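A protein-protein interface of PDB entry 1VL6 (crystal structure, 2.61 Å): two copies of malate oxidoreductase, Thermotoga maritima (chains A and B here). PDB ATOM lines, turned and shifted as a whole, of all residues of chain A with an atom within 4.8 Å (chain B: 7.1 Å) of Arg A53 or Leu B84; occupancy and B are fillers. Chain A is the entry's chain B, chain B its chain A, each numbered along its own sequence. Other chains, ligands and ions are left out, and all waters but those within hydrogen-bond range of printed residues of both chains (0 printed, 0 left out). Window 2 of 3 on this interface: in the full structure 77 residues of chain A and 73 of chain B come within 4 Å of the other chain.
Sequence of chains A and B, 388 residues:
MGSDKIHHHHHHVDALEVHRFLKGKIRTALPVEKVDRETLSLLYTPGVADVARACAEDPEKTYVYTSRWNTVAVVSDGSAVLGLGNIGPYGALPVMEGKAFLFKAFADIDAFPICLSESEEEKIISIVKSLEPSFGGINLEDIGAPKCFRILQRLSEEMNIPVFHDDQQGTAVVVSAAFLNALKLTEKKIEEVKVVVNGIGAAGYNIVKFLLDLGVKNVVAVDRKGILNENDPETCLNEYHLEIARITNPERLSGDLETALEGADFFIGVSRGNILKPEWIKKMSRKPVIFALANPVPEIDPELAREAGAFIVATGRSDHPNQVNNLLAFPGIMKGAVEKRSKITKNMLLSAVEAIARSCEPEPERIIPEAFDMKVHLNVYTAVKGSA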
ATOM      1  N   ALA A  49     -12.098  -0.361 -29.329  1.00  0.00           N
ATOM      2  CA  ALA A  49     -10.687  -0.544 -29.666  1.00  0.00           C
ATOM      3  C   ALA A  49      -9.973   0.779 -29.968  1.00  0.00           C
ATOM      4  O   ALA A  49      -8.816   0.945 -29.582  1.00  0.00           O
ATOM      5  CB  ALA A  49     -10.530  -1.513 -30.810  1.00  0.00           C
ATOM      6  N   ASP A  50     -10.665   1.713 -30.624  1.00  0.00           N
ATOM      7  CA  ASP A  50     -10.103   3.063 -30.841  1.00  0.00           C
ATOM      8  C   ASP A  50      -9.748   3.776 -29.535  1.00  0.00           C
ATOM      9  O   ASP A  50      -8.737   4.465 -29.444  1.00  0.00           O
ATOM     10  CB  ASP A  50     -11.097   3.957 -31.571  1.00  0.00           C
ATOM     11  CG  ASP A  50     -11.412   3.491 -32.981  1.00  0.00           C
ATOM     12  OD1 ASP A  50     -10.493   2.983 -33.673  1.00  0.00           O
ATOM     13  OD2 ASP A  50     -12.558   3.644 -33.472  1.00  0.00           O
ATOM     14  N   VAL A  51     -10.610   3.600 -28.536  1.00  0.00           N
ATOM     15  CA  VAL A  51     -10.457   4.254 -27.257  1.00  0.00           C
ATOM     16  C   VAL A  51      -9.341   3.570 -26.512  1.00  0.00           C
ATOM     17  O   VAL A  51      -8.571   4.221 -25.823  1.00  0.00           O
ATOM     18  CB  VAL A  51     -11.754   4.171 -26.400  1.00  0.00           C
ATOM     19  CG1 VAL A  51     -11.716   5.097 -25.220  1.00  0.00           C
ATOM     20  CG2 VAL A  51     -12.988   4.450 -27.240  1.00  0.00           C
ATOM     21  N   ALA A  52      -9.232   2.253 -26.655  1.00  0.00           N
ATOM     22  CA  ALA A  52      -8.112   1.523 -26.065  1.00  0.00           C
ATOM     23  C   ALA A  52      -6.781   2.009 -26.608  1.00  0.00           C
ATOM     24  O   ALA A  52      -5.893   2.357 -25.838  1.00  0.00           O
ATOM     25  CB  ALA A  52      -8.238   0.030 -26.317  1.00  0.00           C
ATOM     26  N   ARG A  53      -6.655   2.011 -27.932  1.00  0.00           N
ATOM     27  CA  ARG A  53      -5.459   2.509 -28.604  1.00  0.00           C
ATOM     28  C   ARG A  53      -5.084   3.900 -28.091  1.00  0.00           C
ATOM     29  O   ARG A  53      -3.932   4.146 -27.703  1.00  0.00           O
ATOM     30  CB  ARG A  53      -5.637   2.584 -30.109  1.00  0.00           C
ATOM     31  CG  ARG A  53      -5.527   1.262 -30.839  1.00  0.00           C
ATOM     32  CD  ARG A  53      -5.277   1.379 -32.367  1.00  0.00           C
ATOM     33  NE  ARG A  53      -5.903   0.226 -32.979  1.00  0.00           N
ATOM     34  CZ  ARG A  53      -7.214   0.138 -33.275  1.00  0.00           C
ATOM     35  NH1 ARG A  53      -8.039   1.172 -33.085  1.00  0.00           N
ATOM     36  NH2 ARG A  53      -7.710  -0.986 -33.792  1.00  0.00           N
ATOM     37  N   ALA A  54      -6.058   4.791 -28.059  1.00  0.00           N
ATOM     38  CA  ALA A  54      -5.818   6.151 -27.571  1.00  0.00           C
ATOM     39  C   ALA A  54      -5.298   6.202 -26.136  1.00  0.00           C
ATOM     40  O   ALA A  54      -4.406   7.000 -25.844  1.00  0.00           O
ATOM     41  CB  ALA A  54      -7.068   6.999 -27.709  1.00  0.00           C
ATOM     42  N   CYS A  55      -5.846   5.379 -25.248  1.00  0.00           N
ATOM     43  CA  CYS A  55      -5.408   5.393 -23.832  1.00  0.00           C
ATOM     44  C   CYS A  55      -4.065   4.731 -23.587  1.00  0.00           C
ATOM     45  O   CYS A  55      -3.289   5.144 -22.734  1.00  0.00           O
ATOM     46  CB  CYS A  55      -6.432   4.720 -22.932  1.00  0.00           C
ATOM     47  SG  CYS A  55      -7.883   5.767 -22.915  1.00  0.00           S
ATOM     48  N   ALA A  56      -3.785   3.706 -24.361  1.00  0.00           N
ATOM     49  CA  ALA A  56      -2.483   3.088 -24.309  1.00  0.00           C
ATOM     50  C   ALA A  56      -1.418   4.075 -24.776  1.00  0.00           C
ATOM     51  O   ALA A  56      -0.424   4.267 -24.099  1.00  0.00           O
ATOM     52  CB  ALA A  56      -2.452   1.870 -25.157  1.00  0.00           C
ATOM     53  N   GLU A  57      -1.642   4.717 -25.923  1.00  0.00           N
ATOM     54  CA  GLU A  57      -0.669   5.690 -26.453  1.00  0.00           C
ATOM     55  C   GLU A  57      -0.536   6.889 -25.517  1.00  0.00           C
ATOM     56  O   GLU A  57       0.527   7.471 -25.423  1.00  0.00           O
ATOM     57  CB  GLU A  57      -0.975   6.058 -27.888  1.00  0.00           C
ATOM     58  CG  GLU A  57      -0.820   4.847 -28.826  1.00  0.00           C
ATOM     59  CD  GLU A  57      -1.641   4.970 -30.123  1.00  0.00           C
ATOM     60  OE1 GLU A  57      -1.686   6.100 -30.684  1.00  0.00           O
ATOM     61  OE2 GLU A  57      -2.233   3.944 -30.586  1.00  0.00           O
ATOM     62  N   SER B  79      -2.567  -7.361 -20.593  1.00  0.00           N
ATOM     63  CA  SER B  79      -1.548  -8.110 -21.306  1.00  0.00           C
ATOM     64  C   SER B  79      -2.104  -8.737 -22.578  1.00  0.00           C
ATOM     65  O   SER B  79      -1.387  -9.217 -23.391  1.00  0.00           O
ATOM     66  CB  SER B  79      -0.892  -9.155 -20.374  1.00  0.00           C
ATOM     67  OG  SER B  79      -1.806 -10.058 -19.759  1.00  0.00           O
ATOM     68  N   ALA B  80      -3.410  -8.746 -22.743  1.00  0.00           N
ATOM     69  CA  ALA B  80      -4.033  -9.276 -23.976  1.00  0.00           C
ATOM     70  C   ALA B  80      -5.378  -8.632 -24.236  1.00  0.00           C
ATOM     71  O   ALA B  80      -6.437  -9.278 -24.111  1.00  0.00           O
ATOM     72  CB  ALA B  80      -4.206 -10.782 -23.891  1.00  0.00           C
ATOM     73  N   VAL B  81      -5.354  -7.360 -24.624  1.00  0.00           N
ATOM     74  CA  VAL B  81      -6.605  -6.648 -24.829  1.00  0.00           C
ATOM     75  C   VAL B  81      -7.152  -6.923 -26.218  1.00  0.00           C
ATOM     76  O   VAL B  81      -6.507  -6.685 -27.240  1.00  0.00           O
ATOM     77  CB  VAL B  81      -6.513  -5.131 -24.633  1.00  0.00           C
ATOM     78  CG1 VAL B  81      -7.888  -4.470 -24.901  1.00  0.00           C
ATOM     79  CG2 VAL B  81      -6.073  -4.819 -23.238  1.00  0.00           C
ATOM     80  N   LEU B  82      -8.378  -7.391 -26.241  1.00  0.00           N
ATOM     81  CA  LEU B  82      -9.106  -7.582 -27.501  1.00  0.00           C
ATOM     82  C   LEU B  82      -8.158  -8.236 -28.484  1.00  0.00           C
ATOM     83  O   LEU B  82      -7.505  -9.194 -28.124  1.00  0.00           O
ATOM     84  CB  LEU B  82      -9.673  -6.238 -28.023  1.00  0.00           C
ATOM     85  CG  LEU B  82     -10.619  -5.459 -27.083  1.00  0.00           C
ATOM     86  CD1 LEU B  82     -11.053  -4.164 -27.709  1.00  0.00           C
ATOM     87  CD2 LEU B  82     -11.851  -6.291 -26.705  1.00  0.00           C
ATOM     88  N   GLY B  83      -8.039  -7.678 -29.692  1.00  0.00           N
ATOM     89  CA  GLY B  83      -7.108  -8.130 -30.685  1.00  0.00           C
ATOM     90  C   GLY B  83      -5.828  -7.347 -30.688  1.00  0.00           C
ATOM     91  O   GLY B  83      -4.994  -7.578 -31.566  1.00  0.00           O
ATOM     92  N   LEU B  84      -5.645  -6.463 -29.706  1.00  0.00           N
ATOM     93  CA  LEU B  84      -4.562  -5.473 -29.736  1.00  0.00           C
ATOM     94  C   LEU B  84      -3.271  -5.941 -29.105  1.00  0.00           C
ATOM     95  O   LEU B  84      -2.203  -5.390 -29.409  1.00  0.00           O
ATOM     96  CB  LEU B  84      -5.026  -4.207 -29.025  1.00  0.00           C
ATOM     97  CG  LEU B  84      -6.280  -3.620 -29.647  1.00  0.00           C
ATOM     98  CD1 LEU B  84      -6.952  -2.552 -28.784  1.00  0.00           C
ATOM     99  CD2 LEU B  84      -5.918  -3.098 -31.047  1.00  0.00           C
ATOM    100  N   GLY B  85      -3.364  -6.913 -28.200  1.00  0.00           N
ATOM    101  CA  GLY B  85      -2.192  -7.404 -27.464  1.00  0.00           C
ATOM    102  C   GLY B  85      -1.887  -6.729 -26.134  1.00  0.00           C
ATOM    103  O   GLY B  85      -2.773  -6.340 -25.358  1.00  0.00           O
ATOM    104  N   ASN B  86      -0.612  -6.597 -25.863  1.00  0.00           N
ATOM    105  CA  ASN B  86      -0.165  -6.218 -24.544  1.00  0.00           C
ATOM    106  C   ASN B  86      -0.022  -4.692 -24.465  1.00  0.00           C
ATOM    107  O   ASN B  86       1.079  -4.142 -24.477  1.00  0.00           O
ATOM    108  CB  ASN B  86       1.106  -7.006 -24.286  1.00  0.00           C
ATOM    109  CG  ASN B  86       1.776  -6.637 -23.038  1.00  0.00           C
ATOM    110  OD1 ASN B  86       1.111  -6.354 -22.016  1.00  0.00           O
ATOM    111  ND2 ASN B  86       3.151  -6.644 -23.081  1.00  0.00           N
ATOM    112  N   ILE B  87      -1.181  -4.021 -24.408  1.00  0.00           N
ATOM    113  CA  ILE B  87      -1.217  -2.561 -24.423  1.00  0.00           C
ATOM    114  C   ILE B  87      -1.210  -1.969 -23.021  1.00  0.00           C
ATOM    115  O   ILE B  87      -1.019  -0.748 -22.877  1.00  0.00           O
ATOM    116  CB  ILE B  87      -2.466  -2.028 -25.209  1.00  0.00           C
ATOM    117  CG1 ILE B  87      -3.767  -2.331 -24.460  1.00  0.00           C
ATOM    118  CG2 ILE B  87      -2.526  -2.636 -26.568  1.00  0.00           C
ATOM    119  CD1 ILE B  87      -5.050  -2.071 -25.296  1.00  0.00           C
ATOM    120  N   GLY B  91      -4.934   1.264 -21.554  1.00  0.00           N
ATOM    121  CA  GLY B  91      -5.629   0.898 -22.745  1.00  0.00           C
ATOM    122  C   GLY B  91      -6.737  -0.026 -22.359  1.00  0.00           C
ATOM    123  O   GLY B  91      -7.783  -0.018 -22.996  1.00  0.00           O
ATOM    124  N   PRO B  94     -10.915   1.419 -20.682  1.00  0.00           N
ATOM    125  CA  PRO B  94     -12.169   1.651 -21.377  1.00  0.00           C
ATOM    126  C   PRO B  94     -12.804   0.335 -21.842  1.00  0.00           C
ATOM    127  O   PRO B  94     -14.031   0.245 -21.990  1.00  0.00           O
ATOM    128  CB  PRO B  94     -11.763   2.535 -22.541  1.00  0.00           C
ATOM    129  CG  PRO B  94     -10.373   2.238 -22.730  1.00  0.00           C
ATOM    130  CD  PRO B  94      -9.791   1.988 -21.425  1.00  0.00           C
ATOM    131  N   VAL B  95     -11.981  -0.682 -22.030  1.00  0.00           N
ATOM    132  CA  VAL B  95     -12.505  -1.977 -22.389  1.00  0.00           C
ATOM    133  C   VAL B  95     -13.178  -2.623 -21.165  1.00  0.00           C
ATOM    134  O   VAL B  95     -14.295  -3.129 -21.234  1.00  0.00           O
ATOM    135  CB  VAL B  95     -11.409  -2.861 -23.021  1.00  0.00           C
ATOM    136  CG1 VAL B  95     -11.981  -4.154 -23.475  1.00  0.00           C
ATOM    137  CG2 VAL B  95     -10.762  -2.118 -24.210  1.00  0.00           C
ATOM    138  N   ASN B 295      -9.957 -12.913 -34.143  1.00  0.00           N
ATOM    139  CA  ASN B 295     -10.469 -11.580 -33.977  1.00  0.00           C
ATOM    140  C   ASN B 295      -9.352 -10.589 -34.218  1.00  0.00           C
ATOM    141  O   ASN B 295      -8.302 -10.679 -33.594  1.00  0.00           O
ATOM    142  CB  ASN B 295     -11.113 -11.500 -32.561  1.00  0.00           C
ATOM    143  CG  ASN B 295     -10.798 -10.213 -31.791  1.00  0.00           C
ATOM    144  OD1 ASN B 295     -10.846  -9.119 -32.339  1.00  0.00           O
ATOM    145  ND2 ASN B 295     -10.530 -10.355 -30.487  1.00  0.00           N
ATOM    146  N   PRO B 296      -9.564  -9.610 -35.082  1.00  0.00           N
ATOM    147  CA  PRO B 296     -10.825  -9.327 -35.701  1.00  0.00           C
ATOM    148  C   PRO B 296     -11.037  -9.880 -37.108  1.00  0.00           C
ATOM    149  O   PRO B 296     -12.191  -9.859 -37.555  1.00  0.00           O
ATOM    150  CB  PRO B 296     -10.813  -7.792 -35.751  1.00  0.00           C
ATOM    151  CG  PRO B 296      -9.408  -7.455 -35.956  1.00  0.00           C
ATOM    152  CD  PRO B 296      -8.562  -8.598 -35.450  1.00  0.00           C
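Arg A53 touches one residue of chain B. Leu B84 touches just these residues of chain A: Ala A52 (3.8 Å) and Arg A53 (3.8 Å). Of the printed residues of chain B, Ala A52 touches Leu B84 (3.8 Å), Ile B87 (3.95 Å), Gly B91 (3.4 Å) and Val B95 (3.9 Å). Of the printed residues of chain B, Cys A55 touches Gly B91. Of the printed residues of chain B, Val A51 touches Pro B94 (3.7 Å). Printed residues of chain A within 4 Å of Ile B87: Ala A52 (3.95 Å) and Ala A56 (3.8 Å). Asn B86 touches none of the printed residues of chain A. Ala A49 touches none of the printed residues of chain B. The nearest residue of chain A that does not touch Leu B84 is Ala A49 (4.04 Å).
NH1 of Arg A53 is in salt-bridge range of OD1 of Asp A50, at 3.1 Å. The backbone carbonyl oxygen (O) of Val A51 sits at hydrogen-bond distance from the side-chain sulfur (SG) of Cys A55.
CB of Pro B94 touches CG1 of Val A51, at 3.7 Å. Leu B84 touches Ala A52 (CD1 to CB, 3.8 Å). CD1 of Ile B87 touches CB of Ala A52, 3.95 Å away. Gly B91 touches Ala A52 (O to CB, 3.4 Å). CG2 of Val B95 touches CB of Ala A52 (3.9 Å). Arg A53 touches Leu B84 (NE to CD2, 3.8 Å). Gly B91 touches Cys A55. Ile B87 touches Ala A56. Gly B91 touches Ala A56.
No position is printed for both chains. Of the 9 pairs that touch across the chains among the printed residues, none has its exchanged pair printed and touching as well.
Hydrophobic or aromatic side chains of chain A within 4 Å of the printed part of chain B: Val A51, Ala A52 and Ala A56. Among the printed residues, 9 pairs touch across the chains. Among the printed residues, no Asp or Glu carboxylate lies within 4 Å of a Lys or Arg side-chain nitrogen of the other chain.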
